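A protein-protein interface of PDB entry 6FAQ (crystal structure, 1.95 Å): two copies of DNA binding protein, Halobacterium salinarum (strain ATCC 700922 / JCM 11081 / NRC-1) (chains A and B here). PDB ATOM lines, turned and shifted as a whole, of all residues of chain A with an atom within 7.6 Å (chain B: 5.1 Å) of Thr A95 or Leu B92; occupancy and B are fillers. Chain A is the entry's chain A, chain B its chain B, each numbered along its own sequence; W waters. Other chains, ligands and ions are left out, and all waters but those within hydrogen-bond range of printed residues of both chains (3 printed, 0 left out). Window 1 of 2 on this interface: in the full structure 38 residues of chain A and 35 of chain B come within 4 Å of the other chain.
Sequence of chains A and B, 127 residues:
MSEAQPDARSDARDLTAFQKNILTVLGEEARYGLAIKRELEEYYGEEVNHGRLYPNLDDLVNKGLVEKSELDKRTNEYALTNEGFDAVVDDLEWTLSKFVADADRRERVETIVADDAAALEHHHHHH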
ATOM      1  N   TYR A  43     -23.597  -8.559 -33.608  1.00  0.00           N
ATOM      2  CA  TYR A  43     -23.287  -7.146 -33.422  1.00  0.00           C
ATOM      3  C   TYR A  43     -24.098  -6.276 -34.376  1.00  0.00           C
ATOM      4  O   TYR A  43     -24.786  -5.339 -33.952  1.00  0.00           O
ATOM      5  CB  TYR A  43     -21.791  -6.908 -33.622  1.00  0.00           C
ATOM      6  CG  TYR A  43     -21.426  -5.445 -33.708  1.00  0.00           C
ATOM      7  CD1 TYR A  43     -21.307  -4.673 -32.561  1.00  0.00           C
ATOM      8  CD2 TYR A  43     -21.205  -4.836 -34.935  1.00  0.00           C
ATOM      9  CE1 TYR A  43     -20.976  -3.334 -32.633  1.00  0.00           C
ATOM     10  CE2 TYR A  43     -20.872  -3.493 -35.017  1.00  0.00           C
ATOM     11  CZ  TYR A  43     -20.760  -2.749 -33.863  1.00  0.00           C
ATOM     12  OH  TYR A  43     -20.431  -1.413 -33.932  1.00  0.00           O
ATOM     13  N   VAL A  88      -5.786  -3.406 -31.164  1.00  0.00           N
ATOM     14  CA  VAL A  88      -7.005  -3.364 -30.364  1.00  0.00           C
ATOM     15  C   VAL A  88      -6.809  -2.474 -29.142  1.00  0.00           C
ATOM     16  O   VAL A  88      -7.678  -1.661 -28.805  1.00  0.00           O
ATOM     17  CB  VAL A  88      -7.425  -4.790 -29.966  1.00  0.00           C
ATOM     18  CG1 VAL A  88      -8.577  -4.752 -28.971  1.00  0.00           C
ATOM     19  CG2 VAL A  88      -7.804  -5.592 -31.205  1.00  0.00           C
ATOM     20  N   VAL A  89      -5.672  -2.613 -28.459  1.00  0.00           N
ATOM     21  CA  VAL A  89      -5.411  -1.796 -27.279  1.00  0.00           C
ATOM     22  C   VAL A  89      -5.258  -0.330 -27.668  1.00  0.00           C
ATOM     23  O   VAL A  89      -5.704   0.568 -26.944  1.00  0.00           O
ATOM     24  CB  VAL A  89      -4.167  -2.314 -26.537  1.00  0.00           C
ATOM     25  CG1 VAL A  89      -3.811  -1.389 -25.380  1.00  0.00           C
ATOM     26  CG2 VAL A  89      -4.401  -3.728 -26.035  1.00  0.00           C
ATOM     27  N   ASP A  90      -4.625  -0.067 -28.813  1.00  0.00           N
ATOM     28  CA  ASP A  90      -4.398   1.310 -29.238  1.00  0.00           C
ATOM     29  C   ASP A  90      -5.717   2.045 -29.442  1.00  0.00           C
ATOM     30  O   ASP A  90      -5.903   3.160 -28.942  1.00  0.00           O
ATOM     31  CB  ASP A  90      -3.568   1.325 -30.522  1.00  0.00           C
ATOM     32  CG  ASP A  90      -3.409   2.718 -31.095  1.00  0.00           C
ATOM     33  OD1 ASP A  90      -2.723   3.547 -30.462  1.00  0.00           O
ATOM     34  OD2 ASP A  90      -3.970   2.982 -32.180  1.00  0.00           O
ATOM     35  N   ASP A  91      -6.648   1.434 -30.177  1.00  0.00           N
ATOM     36  CA  ASP A  91      -7.935   2.079 -30.411  1.00  0.00           C
ATOM     37  C   ASP A  91      -8.749   2.187 -29.130  1.00  0.00           C
ATOM     38  O   ASP A  91      -9.481   3.165 -28.946  1.00  0.00           O
ATOM     39  CB  ASP A  91      -8.722   1.320 -31.478  1.00  0.00           C
ATOM     40  CG  ASP A  91      -8.273   1.665 -32.888  1.00  0.00           C
ATOM     41  OD1 ASP A  91      -7.327   2.470 -33.034  1.00  0.00           O
ATOM     42  OD2 ASP A  91      -8.870   1.138 -33.850  1.00  0.00           O
ATOM     43  N   LEU A  92      -8.637   1.202 -28.234  1.00  0.00           N
ATOM     44  CA  LEU A  92      -9.337   1.290 -26.958  1.00  0.00           C
ATOM     45  C   LEU A  92      -8.800   2.443 -26.120  1.00  0.00           C
ATOM     46  O   LEU A  92      -9.576   3.203 -25.529  1.00  0.00           O
ATOM     47  CB  LEU A  92      -9.212  -0.029 -26.195  1.00  0.00           C
ATOM     48  CG  LEU A  92      -9.818  -0.044 -24.790  1.00  0.00           C
ATOM     49  CD1 LEU A  92     -11.282   0.367 -24.826  1.00  0.00           C
ATOM     50  CD2 LEU A  92      -9.665  -1.418 -24.150  1.00  0.00           C
ATOM     51  N   GLU A  93      -7.474   2.591 -26.058  1.00  0.00           N
ATOM     52  CA  GLU A  93      -6.886   3.691 -25.300  1.00  0.00           C
ATOM     53  C   GLU A  93      -7.348   5.039 -25.838  1.00  0.00           C
ATOM     54  O   GLU A  93      -7.669   5.948 -25.064  1.00  0.00           O
ATOM     55  CB  GLU A  93      -5.360   3.592 -25.335  1.00  0.00           C
ATOM     56  CG  GLU A  93      -4.796   2.450 -24.500  1.00  0.00           C
ATOM     57  CD  GLU A  93      -3.295   2.286 -24.660  1.00  0.00           C
ATOM     58  OE1 GLU A  93      -2.742   2.789 -25.660  1.00  0.00           O
ATOM     59  OE2 GLU A  93      -2.669   1.651 -23.784  1.00  0.00           O
ATOM     60  N   TRP A  94      -7.391   5.189 -27.163  1.00  0.00           N
ATOM     61  CA  TRP A  94      -7.836   6.450 -27.743  1.00  0.00           C
ATOM     62  C   TRP A  94      -9.315   6.683 -27.460  1.00  0.00           C
ATOM     63  O   TRP A  94      -9.713   7.778 -27.047  1.00  0.00           O
ATOM     64  CB  TRP A  94      -7.563   6.466 -29.247  1.00  0.00           C
ATOM     65  CG  TRP A  94      -7.861   7.788 -29.886  1.00  0.00           C
ATOM     66  CD1 TRP A  94      -7.112   8.925 -29.802  1.00  0.00           C
ATOM     67  CD2 TRP A  94      -8.990   8.110 -30.707  1.00  0.00           C
ATOM     68  NE1 TRP A  94      -7.705   9.936 -30.519  1.00  0.00           N
ATOM     69  CE2 TRP A  94      -8.858   9.461 -31.086  1.00  0.00           C
ATOM     70  CE3 TRP A  94     -10.096   7.386 -31.160  1.00  0.00           C
ATOM     71  CZ2 TRP A  94      -9.792  10.104 -31.894  1.00  0.00           C
ATOM     72  CZ3 TRP A  94     -11.022   8.026 -31.962  1.00  0.00           C
ATOM     73  CH2 TRP A  94     -10.864   9.372 -32.322  1.00  0.00           C
ATOM     74  N   THR A  95     -10.144   5.656 -27.663  1.00  0.00           N
ATOM     75  CA  THR A  95     -11.565   5.785 -27.367  1.00  0.00           C
ATOM     76  C   THR A  95     -11.787   6.184 -25.913  1.00  0.00           C
ATOM     77  O   THR A  95     -12.613   7.054 -25.619  1.00  0.00           O
ATOM     78  CB  THR A  95     -12.286   4.472 -27.682  1.00  0.00           C
ATOM     79  OG1 THR A  95     -12.191   4.200 -29.085  1.00  0.00           O
ATOM     80  CG2 THR A  95     -13.750   4.548 -27.284  1.00  0.00           C
ATOM     81  N   LEU A  96     -11.050   5.563 -24.988  1.00  0.00           N
ATOM     82  CA  LEU A  96     -11.213   5.893 -23.577  1.00  0.00           C
ATOM     83  C   LEU A  96     -10.640   7.267 -23.251  1.00  0.00           C
ATOM     84  O   LEU A  96     -11.127   7.934 -22.330  1.00  0.00           O
ATOM     85  CB  LEU A  96     -10.552   4.824 -22.706  1.00  0.00           C
ATOM     86  CG  LEU A  96     -11.241   3.458 -22.682  1.00  0.00           C
ATOM     87  CD1 LEU A  96     -10.454   2.476 -21.836  1.00  0.00           C
ATOM     88  CD2 LEU A  96     -12.660   3.588 -22.163  1.00  0.00           C
ATOM     89  N   SER A  97      -9.612   7.708 -23.981  1.00  0.00           N
ATOM     90  CA  SER A  97      -9.065   9.037 -23.736  1.00  0.00           C
ATOM     91  C   SER A  97     -10.078  10.122 -24.073  1.00  0.00           C
ATOM     92  O   SER A  97     -10.065  11.193 -23.455  1.00  0.00           O
ATOM     93  CB  SER A  97      -7.782   9.246 -24.542  1.00  0.00           C
ATOM     94  OG  SER A  97      -8.062   9.461 -25.917  1.00  0.00           O
ATOM     95  N   LYS A  98     -10.961   9.866 -25.036  1.00  0.00           N
ATOM     96  CA  LYS A  98     -11.985  10.834 -25.403  1.00  0.00           C
ATOM     97  C   LYS A  98     -13.252  10.691 -24.572  1.00  0.00           C
ATOM     98  O   LYS A  98     -13.958  11.685 -24.361  1.00  0.00           O
ATOM     99  CB  LYS A  98     -12.335  10.698 -26.888  1.00  0.00           C
ATOM    100  CG  LYS A  98     -11.159  10.918 -27.833  1.00  0.00           C
ATOM    101  CD  LYS A  98     -10.611  12.335 -27.739  1.00  0.00           C
ATOM    102  CE  LYS A  98      -9.458  12.553 -28.706  1.00  0.00           C
ATOM    103  NZ  LYS A  98      -8.867  13.915 -28.568  1.00  0.00           N
ATOM    104  N   PHE A  99     -13.559   9.486 -24.088  1.00  0.00           N
ATOM    105  CA  PHE A  99     -14.809   9.290 -23.364  1.00  0.00           C
ATOM    106  C   PHE A  99     -14.671   9.657 -21.894  1.00  0.00           C
ATOM    107  O   PHE A  99     -15.601  10.216 -21.301  1.00  0.00           O
ATOM    108  CB  PHE A  99     -15.283   7.841 -23.505  1.00  0.00           C
ATOM    109  CG  PHE A  99     -16.654   7.603 -22.943  1.00  0.00           C
ATOM    110  CD1 PHE A  99     -16.817   7.181 -21.636  1.00  0.00           C
ATOM    111  CD2 PHE A  99     -17.783   7.814 -23.719  1.00  0.00           C
ATOM    112  CE1 PHE A  99     -18.078   6.967 -21.114  1.00  0.00           C
ATOM    113  CE2 PHE A  99     -19.047   7.601 -23.201  1.00  0.00           C
ATOM    114  CZ  PHE A  99     -19.193   7.178 -21.898  1.00  0.00           C
ATOM    115  N   VAL A 100     -13.530   9.348 -21.284  1.00  0.00           N
ATOM    116  CA  VAL A 100     -13.322   9.646 -19.872  1.00  0.00           C
ATOM    117  C   VAL A 100     -12.995  11.127 -19.748  1.00  0.00           C
ATOM    118  O   VAL A 100     -11.835  11.507 -19.554  1.00  0.00           O
ATOM    119  CB  VAL A 100     -12.214   8.765 -19.271  1.00  0.00           C
ATOM    120  CG1 VAL A 100     -12.049   9.057 -17.791  1.00  0.00           C
ATOM    121  CG2 VAL A 100     -12.529   7.289 -19.495  1.00  0.00           C
ATOM    122  N   ARG A 105     -18.156  10.263 -16.315  1.00  0.00           N
ATOM    123  CA  ARG A 105     -17.733   9.377 -17.395  1.00  0.00           C
ATOM    124  C   ARG A 105     -16.842   8.264 -16.864  1.00  0.00           C
ATOM    125  O   ARG A 105     -16.997   7.097 -17.246  1.00  0.00           O
ATOM    126  CB  ARG A 105     -17.004  10.177 -18.475  1.00  0.00           C
ATOM    127  CG  ARG A 105     -17.883  11.155 -19.239  1.00  0.00           C
ATOM    128  CD  ARG A 105     -18.796  10.445 -20.229  1.00  0.00           C
ATOM    129  NE  ARG A 105     -19.518  11.396 -21.074  1.00  0.00           N
ATOM    130  CZ  ARG A 105     -19.019  11.953 -22.174  1.00  0.00           C
ATOM    131  NH1 ARG A 105     -17.788  11.660 -22.576  1.00  0.00           N
ATOM    132  NH2 ARG A 105     -19.748  12.809 -22.876  1.00  0.00           N
ATOM    133  N   ARG A 108     -18.833   5.676 -15.068  1.00  0.00           N
ATOM    134  CA  ARG A 108     -19.610   4.860 -15.994  1.00  0.00           C
ATOM    135  C   ARG A 108     -18.770   3.725 -16.564  1.00  0.00           C
ATOM    136  O   ARG A 108     -19.219   2.574 -16.621  1.00  0.00           O
ATOM    137  CB  ARG A 108     -20.163   5.734 -17.119  1.00  0.00           C
ATOM    138  CG  ARG A 108     -20.922   4.960 -18.178  1.00  0.00           C
ATOM    139  CD  ARG A 108     -21.474   5.870 -19.261  1.00  0.00           C
ATOM    140  NE  ARG A 108     -22.640   5.260 -19.892  1.00  0.00           N
ATOM    141  CZ  ARG A 108     -23.823   5.849 -20.043  1.00  0.00           C
ATOM    142  NH1 ARG A 108     -24.021   7.101 -19.646  1.00  0.00           N
ATOM    143  NH2 ARG A 108     -24.812   5.182 -20.616  1.00  0.00           N
ATOM    144  N   VAL A 109     -17.545   4.030 -16.999  1.00  0.00           N
ATOM    145  CA  VAL A 109     -16.694   3.004 -17.590  1.00  0.00           C
ATOM    146  C   VAL A 109     -16.280   1.982 -16.540  1.00  0.00           C
ATOM    147  O   VAL A 109     -16.225   0.778 -16.815  1.00  0.00           O
ATOM    148  CB  VAL A 109     -15.466   3.647 -18.258  1.00  0.00           C
ATOM    149  CG1 VAL A 109     -14.515   2.570 -18.755  1.00  0.00           C
ATOM    150  CG2 VAL A 109     -15.897   4.550 -19.397  1.00  0.00           C
ATOM    151  N   ILE A 112     -19.028  -0.477 -16.049  1.00  0.00           N
ATOM    152  CA  ILE A 112     -19.106  -1.398 -17.180  1.00  0.00           C
ATOM    153  C   ILE A 112     -18.030  -2.468 -17.065  1.00  0.00           C
ATOM    154  O   ILE A 112     -18.304  -3.668 -17.189  1.00  0.00           O
ATOM    155  CB  ILE A 112     -18.990  -0.624 -18.507  1.00  0.00           C
ATOM    156  CG1 ILE A 112     -20.200   0.293 -18.693  1.00  0.00           C
ATOM    157  CG2 ILE A 112     -18.861  -1.591 -19.676  1.00  0.00           C
ATOM    158  CD1 ILE A 112     -20.034   1.309 -19.809  1.00  0.00           C
ATOM    159  N   ASP A 116     -18.710  -6.445 -16.388  1.00  0.00           N
ATOM    160  CA  ASP A 116     -18.276  -7.434 -17.369  1.00  0.00           C
ATOM    161  C   ASP A 116     -17.386  -8.488 -16.722  1.00  0.00           C
ATOM    162  O   ASP A 116     -17.559  -9.690 -16.951  1.00  0.00           O
ATOM    163  CB  ASP A 116     -17.547  -6.745 -18.523  1.00  0.00           C
ATOM    164  CG  ASP A 116     -18.472  -5.894 -19.372  1.00  0.00           C
ATOM    165  OD1 ASP A 116     -19.700  -6.116 -19.321  1.00  0.00           O
ATOM    166  OD2 ASP A 116     -17.972  -5.007 -20.095  1.00  0.00           O
ATOM    167  N   THR B  24     -16.552   9.856 -31.699  1.00  0.00           N
ATOM    168  CA  THR B  24     -15.667   9.725 -30.546  1.00  0.00           C
ATOM    169  C   THR B  24     -15.069  11.072 -30.162  1.00  0.00           C
ATOM    170  O   THR B  24     -14.987  11.409 -28.975  1.00  0.00           O
ATOM    171  CB  THR B  24     -14.560   8.714 -30.847  1.00  0.00           C
ATOM    172  OG1 THR B  24     -15.138   7.428 -31.115  1.00  0.00           O
ATOM    173  CG2 THR B  24     -13.598   8.600 -29.671  1.00  0.00           C
ATOM    174  N   VAL B  88     -22.059   6.181 -29.287  1.00  0.00           N
ATOM    175  CA  VAL B  88     -20.704   6.095 -28.754  1.00  0.00           C
ATOM    176  C   VAL B  88     -20.654   5.105 -27.596  1.00  0.00           C
ATOM    177  O   VAL B  88     -19.784   4.227 -27.545  1.00  0.00           O
ATOM    178  CB  VAL B  88     -20.207   7.489 -28.332  1.00  0.00           C
ATOM    179  CG1 VAL B  88     -18.879   7.383 -27.600  1.00  0.00           C
ATOM    180  CG2 VAL B  88     -20.079   8.401 -29.551  1.00  0.00           C
ATOM    181  N   VAL B  89     -21.590   5.227 -26.651  1.00  0.00           N
ATOM    182  CA  VAL B  89     -21.616   4.318 -25.508  1.00  0.00           C
ATOM    183  C   VAL B  89     -21.884   2.892 -25.967  1.00  0.00           C
ATOM    184  O   VAL B  89     -21.371   1.930 -25.381  1.00  0.00           O
ATOM    185  CB  VAL B  89     -22.672   4.779 -24.483  1.00  0.00           C
ATOM    186  CG1 VAL B  89     -22.791   3.764 -23.354  1.00  0.00           C
ATOM    187  CG2 VAL B  89     -22.321   6.149 -23.939  1.00  0.00           C
ATOM    188  N   ASP B  90     -22.697   2.729 -27.009  1.00  0.00           N
ATOM    189  CA  ASP B  90     -23.021   1.395 -27.499  1.00  0.00           C
ATOM    190  C   ASP B  90     -21.770   0.668 -27.977  1.00  0.00           C
ATOM    191  O   ASP B  90     -21.527  -0.485 -27.605  1.00  0.00           O
ATOM    192  CB  ASP B  90     -24.052   1.495 -28.622  1.00  0.00           C
ATOM    193  CG  ASP B  90     -24.443   0.142 -29.173  1.00  0.00           C
ATOM    194  OD1 ASP B  90     -25.136  -0.611 -28.460  1.00  0.00           O
ATOM    195  OD2 ASP B  90     -24.054  -0.168 -30.319  1.00  0.00           O
ATOM    196  N   ASP B  91     -20.956   1.333 -28.802  1.00  0.00           N
ATOM    197  CA  ASP B  91     -19.750   0.690 -29.317  1.00  0.00           C
ATOM    198  C   ASP B  91     -18.722   0.477 -28.215  1.00  0.00           C
ATOM    199  O   ASP B  91     -18.002  -0.529 -28.218  1.00  0.00           O
ATOM    200  CB  ASP B  91     -19.149   1.521 -30.451  1.00  0.00           C
ATOM    201  CG  ASP B  91     -19.834   1.275 -31.781  1.00  0.00           C
ATOM    202  OD1 ASP B  91     -20.719   0.395 -31.846  1.00  0.00           O
ATOM    203  OD2 ASP B  91     -19.485   1.963 -32.765  1.00  0.00           O
ATOM    204  N   LEU B  92     -18.634   1.411 -27.266  1.00  0.00           N
ATOM    205  CA  LEU B  92     -17.703   1.242 -26.157  1.00  0.00           C
ATOM    206  C   LEU B  92     -18.100   0.054 -25.289  1.00  0.00           C
ATOM    207  O   LEU B  92     -17.240  -0.725 -24.862  1.00  0.00           O
ATOM    208  CB  LEU B  92     -17.644   2.522 -25.324  1.00  0.00           C
ATOM    209  CG  LEU B  92     -16.651   2.515 -24.159  1.00  0.00           C
ATOM    210  CD1 LEU B  92     -15.238   2.264 -24.662  1.00  0.00           C
ATOM    211  CD2 LEU B  92     -16.720   3.824 -23.381  1.00  0.00           C
ATOM    212  N   GLU B  93     -19.398  -0.104 -25.022  1.00  0.00           N
ATOM    213  CA  GLU B  93     -19.861  -1.257 -24.255  1.00  0.00           C
ATOM    214  C   GLU B  93     -19.523  -2.558 -24.972  1.00  0.00           C
ATOM    215  O   GLU B  93     -18.983  -3.491 -24.367  1.00  0.00           O
ATOM    216  CB  GLU B  93     -21.367  -1.154 -24.008  1.00  0.00           C
ATOM    217  CG  GLU B  93     -21.763  -0.088 -22.998  1.00  0.00           C
ATOM    218  CD  GLU B  93     -23.268   0.041 -22.843  1.00  0.00           C
ATOM    219  OE1 GLU B  93     -24.004  -0.708 -23.519  1.00  0.00           O
ATOM    220  OE2 GLU B  93     -23.716   0.890 -22.044  1.00  0.00           O
ATOM    221  N   TRP B  94     -19.830  -2.639 -26.268  1.00  0.00           N
ATOM    222  CA  TRP B  94     -19.519  -3.851 -27.019  1.00  0.00           C
ATOM    223  C   TRP B  94     -18.018  -4.109 -27.025  1.00  0.00           C
ATOM    224  O   TRP B  94     -17.568  -5.239 -26.795  1.00  0.00           O
ATOM    225  CB  TRP B  94     -20.056  -3.744 -28.447  1.00  0.00           C
ATOM    226  CG  TRP B  94     -19.881  -5.011 -29.238  1.00  0.00           C
ATOM    227  CD1 TRP B  94     -20.606  -6.162 -29.116  1.00  0.00           C
ATOM    228  CD2 TRP B  94     -18.916  -5.256 -30.269  1.00  0.00           C
ATOM    229  NE1 TRP B  94     -20.154  -7.107 -30.006  1.00  0.00           N
ATOM    230  CE2 TRP B  94     -19.117  -6.576 -30.726  1.00  0.00           C
ATOM    231  CE3 TRP B  94     -17.904  -4.487 -30.850  1.00  0.00           C
ATOM    232  CZ2 TRP B  94     -18.343  -7.142 -31.736  1.00  0.00           C
ATOM    233  CZ3 TRP B  94     -17.137  -5.050 -31.852  1.00  0.00           C
ATOM    234  CH2 TRP B  94     -17.360  -6.364 -32.286  1.00  0.00           C
ATOM    235  N   THR B  95     -17.224  -3.065 -27.272  1.00  0.00           N
ATOM    236  CA  THR B  95     -15.773  -3.211 -27.255  1.00  0.00           C
ATOM    237  C   THR B  95     -15.286  -3.725 -25.906  1.00  0.00           C
ATOM    238  O   THR B  95     -14.427  -4.612 -25.844  1.00  0.00           O
ATOM    239  CB  THR B  95     -15.113  -1.872 -27.591  1.00  0.00           C
ATOM    240  OG1 THR B  95     -15.313  -1.579 -28.980  1.00  0.00           O
ATOM    241  CG2 THR B  95     -13.625  -1.906 -27.284  1.00  0.00           C
ATOM    242  N   LEU B  96     -15.829  -3.186 -24.813  1.00  0.00           N
ATOM    243  CA  LEU B  96     -15.387  -3.609 -23.489  1.00  0.00           C
ATOM    244  C   LEU B  96     -15.865  -5.021 -23.172  1.00  0.00           C
ATOM    245  O   LEU B  96     -15.149  -5.793 -22.524  1.00  0.00           O
ATOM    246  CB  LEU B  96     -15.879  -2.619 -22.433  1.00  0.00           C
ATOM    247  CG  LEU B  96     -15.204  -1.243 -22.443  1.00  0.00           C
ATOM    248  CD1 LEU B  96     -15.893  -0.298 -21.469  1.00  0.00           C
ATOM    249  CD2 LEU B  96     -13.725  -1.363 -22.108  1.00  0.00           C
ATOM    250  N   SER B  97     -17.070  -5.380 -23.623  1.00  0.00           N
ATOM    251  CA  SER B  97     -17.574  -6.728 -23.373  1.00  0.00           C
ATOM    252  C   SER B  97     -16.662  -7.781 -23.985  1.00  0.00           C
ATOM    253  O   SER B  97     -16.608  -8.915 -23.497  1.00  0.00           O
ATOM    254  CB  SER B  97     -18.991  -6.879 -23.926  1.00  0.00           C
ATOM    255  OG  SER B  97     -18.985  -6.945 -25.344  1.00  0.00           O
HETATM  256  O   HOH W   1     -15.777   9.899 -26.725  1.00  0.00           O
HETATM  257  O   HOH W   2     -23.108   2.806 -19.741  1.00  0.00           O
HETATM  258  O   HOH W   3     -20.000  -4.036 -21.738  1.00  0.00           O
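The side-chain carboxylate (OD1) of Asp B91 sits at hydrogen-bond distance from the side-chain hydroxyl (OH) of Tyr A43 (2.8 Å).
Thr A95 touches Leu B92, but with the chains exchanged Leu A92 does not touch Thr B95 (4.1 Å).
Leu A96 touches Leu B92, but with the chains exchanged Leu A92 does not touch Leu B96 (4.04 Å).
Positions printed for both chains: 88, 89, 90, 91, 92, 93, 94, 95, 96 and 97.
Of the 11 printed residues of chain B, 8 touch a printed residue of chain A.
Hydrophobic or aromatic side chains of chain B that line the printed part of chain A: Val B89, Leu B92, Trp B94 and Leu B96.
The backbone carbonyl oxygen of Asp A91 sits at hydrogen-bond distance from the side-chain hydroxyl of Thr A95, at 2.9 Å.
The backbone carbonyl oxygen of Trp A94 is in hydrogen-bond range of the side-chain hydroxyl of Ser A97 (2.6 Å).
NH1 of Arg A105 is in hydrogen-bond range of O of Phe A99, at 2.9 Å.
O of Asp B91 sits at hydrogen-bond distance from OG1 of Thr B95, 3.0 Å away.
The backbone carbonyl oxygen (O) of Trp B94 is in hydrogen-bond range of the side-chain hydroxyl (OG) of Ser B97 (2.7 Å).
Thr A95 touches just one residue of chain B: Leu B92 (3.8 Å).
Of the printed residues of chain B, Lys A98 touches Thr B24.
Of the printed residues of chain B, Ile A112 touches Glu B93 and Leu B96.
Of the printed residues of chain B, Arg A108 touches Val B89.
Val A109 touches none of the printed residues of chain B.
Val A89 touches none of the printed residues of chain B.
The nearest residue of chain A that does not touch Leu B92 is Val A109 (4.1 Å).
Water W2 lies within hydrogen-bond range of NE of Arg A108 (2.5 Å) and OE2 of Glu B93 (3.1 Å).
Water W3 lies within hydrogen-bond range of OD2 of Asp A116 and O of Glu B93.
Water W1 lies within hydrogen-bond range of O of Thr B24 (2.8 Å), N of Phe A99 (3.5 Å) and O of Lys A98 (3.5 Å).
Among the printed residues, merely in contact across the chains: Tyr A43 with Trp B94, Trp A94 with Thr B24, Thr A95 with Leu B92, Leu A96 with Leu B92, Lys A98 with Thr B24, Phe A99 with Val B89, Phe A99 with Leu B92, Arg A108 with Val B89, Ile A112 with Glu B93, Ile A112 with Leu B96, Asp A116 with Leu B96 and Asp A116 with Ser B97.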
